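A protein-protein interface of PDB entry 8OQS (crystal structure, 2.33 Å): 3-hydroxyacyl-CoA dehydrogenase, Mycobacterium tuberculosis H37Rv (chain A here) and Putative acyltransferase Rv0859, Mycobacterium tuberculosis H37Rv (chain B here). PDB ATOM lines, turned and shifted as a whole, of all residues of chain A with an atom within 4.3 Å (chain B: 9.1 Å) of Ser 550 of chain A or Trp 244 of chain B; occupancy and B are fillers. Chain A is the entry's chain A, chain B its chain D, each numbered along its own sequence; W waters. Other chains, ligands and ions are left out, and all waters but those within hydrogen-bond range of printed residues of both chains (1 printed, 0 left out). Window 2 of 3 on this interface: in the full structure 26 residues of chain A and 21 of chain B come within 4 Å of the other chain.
The backbone carbonyl oxygen (O) of His 243 of chain B sits close to the backbone carbonyl oxygen (O) of Ala 549 of chain A (3.2 Å). A ring nitrogen (ND1) of His 243 of chain B is in hydrogen-bond range of the side-chain hydroxyl of Ser 550 of chain A. The side-chain hydroxyl of Ser 550 of chain A sits close to the backbone NH of Trp 244 of chain B (3.5 Å).
CB of Ala 549 of chain A touches O of Trp 244 of chain B (3.5 Å). Gln 553 of chain A touches Leu 239 of chain B (CD to O, 3.6 Å). CA of Gln 240 of chain B touches OE1 of Gln 553 of chain A, at 3.7 Å. Gln 553 of chain A touches His 243 of chain B. His 243 of chain B touches Leu 648 of chain A (CD2 to CD2, 3.9 Å).
Ser 550 of chain A touches two residues of chain B. Trp 244 of chain B touches two residues of chain A. No residue of chain B comes within 4 Å of Glu 547 of chain A. Of the printed residues of chain A, Gln 240 of chain B touches Gln 553 (3.7 Å). Of the printed residues of chain A, His 243 of chain B touches Ala 549, Ser 550, Gln 553 and Leu 648. Of the printed residues of chain B, Gln 553 of chain A touches Leu 239 (3.6 Å), Gln 240 (3.7 Å) and His 243 (3.6 Å). Of the printed residues of chain B, Leu 648 of chain A touches His 243. Printed residues of chain A within 4 Å of Leu 239 of chain B: Gln 553. Thr 158 of chain B touches none of the printed residues of chain A. Lys 241 of chain B touches none of the printed residues of chain A. The nearest residue of chain B that does not touch Ser 550 of chain A is Val 245 of chain B (5.8 Å). The nearest printed residue of chain B that does not touch Leu 648 of chain A is Gln 240 of chain B (4.6 Å).
Of the 16 printed residues of chain B, 4 touch a printed residue of chain A. Hydrophobic or aromatic side chains of chain A within 4 Å of the printed part of chain B: Ala 549 and Leu 648. Along chain A the printed residues that touch a printed residue of chain B span positions 549 to 648. Among the printed residues, 8 pairs touch across the chains.
Water W1 lies within hydrogen-bond range of OE1 of Glu 547 of chain A (2.8 Å), N of Ala 549 of chain A (3.1 Å) and O of Trp 244 of chain B (3.5 Å).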
ATOM      1  N   GLU A 547      -2.203 -15.078   5.419  1.00  0.00           N
ATOM      2  CA  GLU A 547      -2.194 -16.120   6.439  1.00  0.00           C
ATOM      3  C   GLU A 547      -3.403 -17.037   6.271  1.00  0.00           C
ATOM      4  O   GLU A 547      -4.529 -16.545   6.105  1.00  0.00           O
ATOM      5  CB  GLU A 547      -2.203 -15.502   7.835  1.00  0.00           C
ATOM      6  CG  GLU A 547      -0.922 -14.793   8.219  1.00  0.00           C
ATOM      7  CD  GLU A 547       0.153 -15.752   8.689  1.00  0.00           C
ATOM      8  OE1 GLU A 547      -0.039 -16.979   8.540  1.00  0.00           O
ATOM      9  OE2 GLU A 547       1.184 -15.278   9.216  1.00  0.00           O
ATOM     10  N   PRO A 548      -3.221 -18.361   6.306  1.00  0.00           N
ATOM     11  CA  PRO A 548      -4.385 -19.255   6.179  1.00  0.00           C
ATOM     12  C   PRO A 548      -5.427 -19.021   7.253  1.00  0.00           C
ATOM     13  O   PRO A 548      -6.627 -19.129   6.977  1.00  0.00           O
ATOM     14  CB  PRO A 548      -3.762 -20.656   6.280  1.00  0.00           C
ATOM     15  CG  PRO A 548      -2.327 -20.463   5.894  1.00  0.00           C
ATOM     16  CD  PRO A 548      -1.961 -19.111   6.434  1.00  0.00           C
ATOM     17  N   ALA A 549      -4.999 -18.693   8.476  1.00  0.00           N
ATOM     18  CA  ALA A 549      -5.956 -18.445   9.549  1.00  0.00           C
ATOM     19  C   ALA A 549      -6.812 -17.221   9.252  1.00  0.00           C
ATOM     20  O   ALA A 549      -8.012 -17.207   9.555  1.00  0.00           O
ATOM     21  CB  ALA A 549      -5.222 -18.279  10.879  1.00  0.00           C
ATOM     22  N   SER A 550      -6.214 -16.180   8.666  1.00  0.00           N
ATOM     23  CA  SER A 550      -6.995 -15.014   8.269  1.00  0.00           C
ATOM     24  C   SER A 550      -7.994 -15.373   7.178  1.00  0.00           C
ATOM     25  O   SER A 550      -9.137 -14.898   7.195  1.00  0.00           O
ATOM     26  CB  SER A 550      -6.074 -13.887   7.794  1.00  0.00           C
ATOM     27  OG  SER A 550      -5.370 -13.301   8.876  1.00  0.00           O
ATOM     28  N   ILE A 551      -7.582 -16.216   6.228  1.00  0.00           N
ATOM     29  CA  ILE A 551      -8.486 -16.625   5.158  1.00  0.00           C
ATOM     30  C   ILE A 551      -9.718 -17.303   5.741  1.00  0.00           C
ATOM     31  O   ILE A 551     -10.857 -16.953   5.410  1.00  0.00           O
ATOM     32  CB  ILE A 551      -7.757 -17.536   4.155  1.00  0.00           C
ATOM     33  CG1 ILE A 551      -6.586 -16.790   3.509  1.00  0.00           C
ATOM     34  CG2 ILE A 551      -8.725 -18.037   3.084  1.00  0.00           C
ATOM     35  CD1 ILE A 551      -5.844 -17.596   2.465  1.00  0.00           C
ATOM     36  N   GLU A 552      -9.513 -18.261   6.646  1.00  0.00           N
ATOM     37  CA  GLU A 552     -10.647 -18.991   7.202  1.00  0.00           C
ATOM     38  C   GLU A 552     -11.526 -18.089   8.062  1.00  0.00           C
ATOM     39  O   GLU A 552     -12.756 -18.217   8.045  1.00  0.00           O
ATOM     40  CB  GLU A 552     -10.151 -20.192   8.001  1.00  0.00           C
ATOM     41  CG  GLU A 552      -9.246 -21.133   7.216  1.00  0.00           C
ATOM     42  CD  GLU A 552      -9.980 -21.904   6.127  1.00  0.00           C
ATOM     43  OE1 GLU A 552     -10.351 -21.299   5.098  1.00  0.00           O
ATOM     44  OE2 GLU A 552     -10.186 -23.126   6.300  1.00  0.00           O
ATOM     45  N   GLN A 553     -10.918 -17.173   8.819  1.00  0.00           N
ATOM     46  CA  GLN A 553     -11.710 -16.210   9.578  1.00  0.00           C
ATOM     47  C   GLN A 553     -12.531 -15.324   8.654  1.00  0.00           C
ATOM     48  O   GLN A 553     -13.710 -15.058   8.918  1.00  0.00           O
ATOM     49  CB  GLN A 553     -10.802 -15.356  10.462  1.00  0.00           C
ATOM     50  CG  GLN A 553     -10.408 -16.026  11.760  1.00  0.00           C
ATOM     51  CD  GLN A 553     -11.518 -15.997  12.786  1.00  0.00           C
ATOM     52  OE1 GLN A 553     -12.463 -15.216  12.675  1.00  0.00           O
ATOM     53  NE2 GLN A 553     -11.411 -16.849  13.793  1.00  0.00           N
ATOM     54  N   ALA A 554     -11.923 -14.851   7.565  1.00  0.00           N
ATOM     55  CA  ALA A 554     -12.662 -14.034   6.612  1.00  0.00           C
ATOM     56  C   ALA A 554     -13.859 -14.793   6.056  1.00  0.00           C
ATOM     57  O   ALA A 554     -14.949 -14.226   5.908  1.00  0.00           O
ATOM     58  CB  ALA A 554     -11.737 -13.577   5.488  1.00  0.00           C
ATOM     59  N   LEU A 648      -9.057  -7.279   6.645  1.00  0.00           N
ATOM     60  CA  LEU A 648      -9.976  -8.413   6.671  1.00  0.00           C
ATOM     61  C   LEU A 648     -11.178  -8.167   5.769  1.00  0.00           C
ATOM     62  O   LEU A 648     -11.623  -9.075   5.055  1.00  0.00           O
ATOM     63  CB  LEU A 648     -10.426  -8.700   8.102  1.00  0.00           C
ATOM     64  CG  LEU A 648     -11.193 -10.010   8.284  1.00  0.00           C
ATOM     65  CD1 LEU A 648     -10.305 -11.197   7.949  1.00  0.00           C
ATOM     66  CD2 LEU A 648     -11.754 -10.136   9.697  1.00  0.00           C
ATOM     67  N   MET A 651     -10.556  -9.120   2.248  1.00  0.00           N
ATOM     68  CA  MET A 651     -10.657 -10.562   2.059  1.00  0.00           C
ATOM     69  C   MET A 651     -12.113 -10.999   2.004  1.00  0.00           C
ATOM     70  O   MET A 651     -12.512 -11.763   1.118  1.00  0.00           O
ATOM     71  CB  MET A 651      -9.926 -11.293   3.180  1.00  0.00           C
ATOM     72  CG  MET A 651      -8.445 -11.028   3.233  1.00  0.00           C
ATOM     73  SD  MET A 651      -7.703 -11.988   4.556  1.00  0.00           S
ATOM     74  CE  MET A 651      -7.315 -10.705   5.737  1.00  0.00           C
ATOM     75  N   LEU B 155      -3.178 -14.988  24.975  1.00  0.00           N
ATOM     76  CA  LEU B 155      -2.969 -14.561  23.596  1.00  0.00           C
ATOM     77  C   LEU B 155      -1.600 -13.916  23.423  1.00  0.00           C
ATOM     78  O   LEU B 155      -0.938 -14.118  22.399  1.00  0.00           O
ATOM     79  CB  LEU B 155      -4.083 -13.604  23.173  1.00  0.00           C
ATOM     80  CG  LEU B 155      -4.085 -13.140  21.714  1.00  0.00           C
ATOM     81  CD1 LEU B 155      -4.203 -14.320  20.757  1.00  0.00           C
ATOM     82  CD2 LEU B 155      -5.211 -12.143  21.481  1.00  0.00           C
ATOM     83  N   THR B 158       0.872 -16.621  23.263  1.00  0.00           N
ATOM     84  CA  THR B 158       0.779 -17.321  21.988  1.00  0.00           C
ATOM     85  C   THR B 158       1.517 -16.564  20.894  1.00  0.00           C
ATOM     86  O   THR B 158       2.256 -17.163  20.107  1.00  0.00           O
ATOM     87  CB  THR B 158      -0.686 -17.519  21.602  1.00  0.00           C
ATOM     88  OG1 THR B 158      -1.350 -18.274  22.622  1.00  0.00           O
ATOM     89  CG2 THR B 158      -0.790 -18.263  20.280  1.00  0.00           C
ATOM     90  N   ILE B 159       1.341 -15.245  20.844  1.00  0.00           N
ATOM     91  CA  ILE B 159       1.954 -14.443  19.788  1.00  0.00           C
ATOM     92  C   ILE B 159       3.456 -14.328  20.010  1.00  0.00           C
ATOM     93  O   ILE B 159       4.260 -14.676  19.139  1.00  0.00           O
ATOM     94  CB  ILE B 159       1.285 -13.060  19.714  1.00  0.00           C
ATOM     95  CG1 ILE B 159      -0.187 -13.209  19.326  1.00  0.00           C
ATOM     96  CG2 ILE B 159       2.018 -12.165  18.733  1.00  0.00           C
ATOM     97  CD1 ILE B 159      -0.980 -11.932  19.434  1.00  0.00           C
ATOM     98  N   GLU B 160       3.858 -13.848  21.188  1.00  0.00           N
ATOM     99  CA  GLU B 160       5.275 -13.626  21.454  1.00  0.00           C
ATOM    100  C   GLU B 160       6.065 -14.924  21.572  1.00  0.00           C
ATOM    101  O   GLU B 160       7.299 -14.886  21.519  1.00  0.00           O
ATOM    102  CB  GLU B 160       5.439 -12.793  22.723  1.00  0.00           C
ATOM    103  CG  GLU B 160       4.795 -11.417  22.634  1.00  0.00           C
ATOM    104  CD  GLU B 160       5.473 -10.514  21.617  1.00  0.00           C
ATOM    105  OE1 GLU B 160       6.716 -10.576  21.491  1.00  0.00           O
ATOM    106  OE2 GLU B 160       4.758  -9.745  20.939  1.00  0.00           O
ATOM    107  N   ALA B 238     -11.756 -13.338  20.756  1.00  0.00           N
ATOM    108  CA  ALA B 238     -10.397 -12.822  20.613  1.00  0.00           C
ATOM    109  C   ALA B 238      -9.838 -13.118  19.228  1.00  0.00           C
ATOM    110  O   ALA B 238      -9.219 -12.249  18.603  1.00  0.00           O
ATOM    111  CB  ALA B 238      -9.489 -13.412  21.693  1.00  0.00           C
ATOM    112  N   LEU B 239     -10.052 -14.337  18.725  1.00  0.00           N
ATOM    113  CA  LEU B 239      -9.512 -14.706  17.422  1.00  0.00           C
ATOM    114  C   LEU B 239     -10.276 -14.068  16.269  1.00  0.00           C
ATOM    115  O   LEU B 239      -9.747 -14.001  15.153  1.00  0.00           O
ATOM    116  CB  LEU B 239      -9.506 -16.224  17.259  1.00  0.00           C
ATOM    117  CG  LEU B 239      -8.617 -16.987  18.237  1.00  0.00           C
ATOM    118  CD1 LEU B 239      -8.655 -18.476  17.934  1.00  0.00           C
ATOM    119  CD2 LEU B 239      -7.200 -16.452  18.177  1.00  0.00           C
ATOM    120  N   GLN B 240     -11.510 -13.617  16.497  1.00  0.00           N
ATOM    121  CA  GLN B 240     -12.175 -12.822  15.473  1.00  0.00           C
ATOM    122  C   GLN B 240     -11.466 -11.488  15.281  1.00  0.00           C
ATOM    123  O   GLN B 240     -11.444 -10.953  14.167  1.00  0.00           O
ATOM    124  CB  GLN B 240     -13.647 -12.615  15.831  1.00  0.00           C
ATOM    125  CG  GLN B 240     -14.492 -13.886  15.782  1.00  0.00           C
ATOM    126  CD  GLN B 240     -15.950 -13.624  16.119  1.00  0.00           C
ATOM    127  OE1 GLN B 240     -16.350 -12.480  16.325  1.00  0.00           O
ATOM    128  NE2 GLN B 240     -16.750 -14.685  16.179  1.00  0.00           N
ATOM    129  N   LYS B 241     -10.857 -10.959  16.347  1.00  0.00           N
ATOM    130  CA  LYS B 241     -10.057  -9.740  16.252  1.00  0.00           C
ATOM    131  C   LYS B 241      -8.664 -10.032  15.703  1.00  0.00           C
ATOM    132  O   LYS B 241      -8.198  -9.355  14.781  1.00  0.00           O
ATOM    133  CB  LYS B 241      -9.965  -9.074  17.626  1.00  0.00           C
ATOM    134  CG  LYS B 241      -9.010  -7.896  17.701  1.00  0.00           C
ATOM    135  CD  LYS B 241      -9.625  -6.637  17.131  1.00  0.00           C
ATOM    136  CE  LYS B 241      -8.649  -5.477  17.220  1.00  0.00           C
ATOM    137  NZ  LYS B 241      -9.240  -4.198  16.739  1.00  0.00           N
ATOM    138  N   TYR B 242      -7.994 -11.044  16.254  1.00  0.00           N
ATOM    139  CA  TYR B 242      -6.640 -11.415  15.841  1.00  0.00           C
ATOM    140  C   TYR B 242      -6.705 -12.611  14.892  1.00  0.00           C
ATOM    141  O   TYR B 242      -6.271 -13.723  15.199  1.00  0.00           O
ATOM    142  CB  TYR B 242      -5.782 -11.712  17.067  1.00  0.00           C
ATOM    143  CG  TYR B 242      -5.549 -10.495  17.927  1.00  0.00           C
ATOM    144  CD1 TYR B 242      -6.466 -10.126  18.908  1.00  0.00           C
ATOM    145  CD2 TYR B 242      -4.422  -9.700  17.745  1.00  0.00           C
ATOM    146  CE1 TYR B 242      -6.262  -9.003  19.689  1.00  0.00           C
ATOM    147  CE2 TYR B 242      -4.210  -8.577  18.520  1.00  0.00           C
ATOM    148  CZ  TYR B 242      -5.132  -8.233  19.489  1.00  0.00           C
ATOM    149  OH  TYR B 242      -4.917  -7.114  20.259  1.00  0.00           O
ATOM    150  N   HIS B 243      -7.243 -12.343  13.700  1.00  0.00           N
ATOM    151  CA  HIS B 243      -7.625 -13.406  12.775  1.00  0.00           C
ATOM    152  C   HIS B 243      -6.441 -14.181  12.211  1.00  0.00           C
ATOM    153  O   HIS B 243      -6.653 -15.261  11.643  1.00  0.00           O
ATOM    154  CB  HIS B 243      -8.460 -12.826  11.633  1.00  0.00           C
ATOM    155  CG  HIS B 243      -7.885 -11.586  11.024  1.00  0.00           C
ATOM    156  ND1 HIS B 243      -6.863 -11.614  10.097  1.00  0.00           N
ATOM    157  CD2 HIS B 243      -8.198 -10.280  11.198  1.00  0.00           C
ATOM    158  CE1 HIS B 243      -6.571 -10.380   9.730  1.00  0.00           C
ATOM    159  NE2 HIS B 243      -7.367  -9.551  10.384  1.00  0.00           N
ATOM    160  N   TRP B 244      -5.214 -13.678  12.351  1.00  0.00           N
ATOM    161  CA  TRP B 244      -4.055 -14.418  11.865  1.00  0.00           C
ATOM    162  C   TRP B 244      -3.565 -15.466  12.859  1.00  0.00           C
ATOM    163  O   TRP B 244      -2.774 -16.336  12.478  1.00  0.00           O
ATOM    164  CB  TRP B 244      -2.920 -13.449  11.517  1.00  0.00           C
ATOM    165  CG  TRP B 244      -2.461 -12.617  12.668  1.00  0.00           C
ATOM    166  CD1 TRP B 244      -1.441 -12.903  13.529  1.00  0.00           C
ATOM    167  CD2 TRP B 244      -3.002 -11.360  13.091  1.00  0.00           C
ATOM    168  NE1 TRP B 244      -1.315 -11.902  14.462  1.00  0.00           N
ATOM    169  CE2 TRP B 244      -2.262 -10.943  14.215  1.00  0.00           C
ATOM    170  CE3 TRP B 244      -4.042 -10.548  12.631  1.00  0.00           C
ATOM    171  CZ2 TRP B 244      -2.528  -9.752  14.883  1.00  0.00           C
ATOM    172  CZ3 TRP B 244      -4.303  -9.362  13.297  1.00  0.00           C
ATOM    173  CH2 TRP B 244      -3.550  -8.976  14.409  1.00  0.00           C
ATOM    174  N   VAL B 245      -4.016 -15.407  14.108  1.00  0.00           N
ATOM    175  CA  VAL B 245      -3.698 -16.418  15.110  1.00  0.00           C
ATOM    176  C   VAL B 245      -4.719 -17.544  15.001  1.00  0.00           C
ATOM    177  O   VAL B 245      -5.932 -17.297  14.990  1.00  0.00           O
ATOM    178  CB  VAL B 245      -3.698 -15.808  16.522  1.00  0.00           C
ATOM    179  CG1 VAL B 245      -3.427 -16.878  17.565  1.00  0.00           C
ATOM    180  CG2 VAL B 245      -2.671 -14.694  16.618  1.00  0.00           C
ATOM    181  N   GLU B 246      -4.235 -18.784  14.927  1.00  0.00           N
ATOM    182  CA  GLU B 246      -5.119 -19.929  14.742  1.00  0.00           C
ATOM    183  C   GLU B 246      -5.634 -20.493  16.062  1.00  0.00           C
ATOM    184  O   GLU B 246      -6.832 -20.765  16.198  1.00  0.00           O
ATOM    185  CB  GLU B 246      -4.396 -21.023  13.954  1.00  0.00           C
ATOM    186  CG  GLU B 246      -5.267 -22.228  13.648  1.00  0.00           C
ATOM    187  CD  GLU B 246      -4.506 -23.326  12.944  1.00  0.00           C
ATOM    188  OE1 GLU B 246      -3.307 -23.124  12.662  1.00  0.00           O
ATOM    189  OE2 GLU B 246      -5.104 -24.390  12.677  1.00  0.00           O
ATOM    190  N   LYS B 247      -4.745 -20.689  17.033  1.00  0.00           N
ATOM    191  CA  LYS B 247      -5.097 -21.298  18.307  1.00  0.00           C
ATOM    192  C   LYS B 247      -4.427 -20.522  19.431  1.00  0.00           C
ATOM    193  O   LYS B 247      -3.267 -20.115  19.306  1.00  0.00           O
ATOM    194  CB  LYS B 247      -4.674 -22.776  18.352  1.00  0.00           C
ATOM    195  CG  LYS B 247      -4.920 -23.476  19.685  1.00  0.00           C
ATOM    196  CD  LYS B 247      -6.364 -23.929  19.829  1.00  0.00           C
ATOM    197  CE  LYS B 247      -6.608 -25.245  19.103  1.00  0.00           C
ATOM    198  NZ  LYS B 247      -5.862 -26.376  19.728  1.00  0.00           N
ATOM    199  N   ASP B 295      -4.596  -2.146  22.318  1.00  0.00           N
ATOM    200  CA  ASP B 295      -5.858  -2.765  21.934  1.00  0.00           C
ATOM    201  C   ASP B 295      -6.553  -3.377  23.151  1.00  0.00           C
ATOM    202  O   ASP B 295      -5.899  -4.023  23.980  1.00  0.00           O
ATOM    203  CB  ASP B 295      -5.621  -3.835  20.867  1.00  0.00           C
ATOM    204  CG  ASP B 295      -6.911  -4.327  20.237  1.00  0.00           C
ATOM    205  OD1 ASP B 295      -7.590  -3.523  19.563  1.00  0.00           O
ATOM    206  OD2 ASP B 295      -7.248  -5.516  20.419  1.00  0.00           O
ATOM    207  N   ILE B 298      -6.310  -7.665  23.501  1.00  0.00           N
ATOM    208  CA  ILE B 298      -5.059  -8.092  24.120  1.00  0.00           C
ATOM    209  C   ILE B 298      -4.896  -7.417  25.479  1.00  0.00           C
ATOM    210  O   ILE B 298      -4.318  -8.001  26.405  1.00  0.00           O
ATOM    211  CB  ILE B 298      -3.878  -7.817  23.166  1.00  0.00           C
ATOM    212  CG1 ILE B 298      -2.906  -8.996  23.136  1.00  0.00           C
ATOM    213  CG2 ILE B 298      -3.147  -6.534  23.526  1.00  0.00           C
ATOM    214  CD1 ILE B 298      -1.751  -8.792  22.176  1.00  0.00           C
HETATM  215  O   HOH W   1      -2.144 -18.332   9.684  1.00  0.00           O
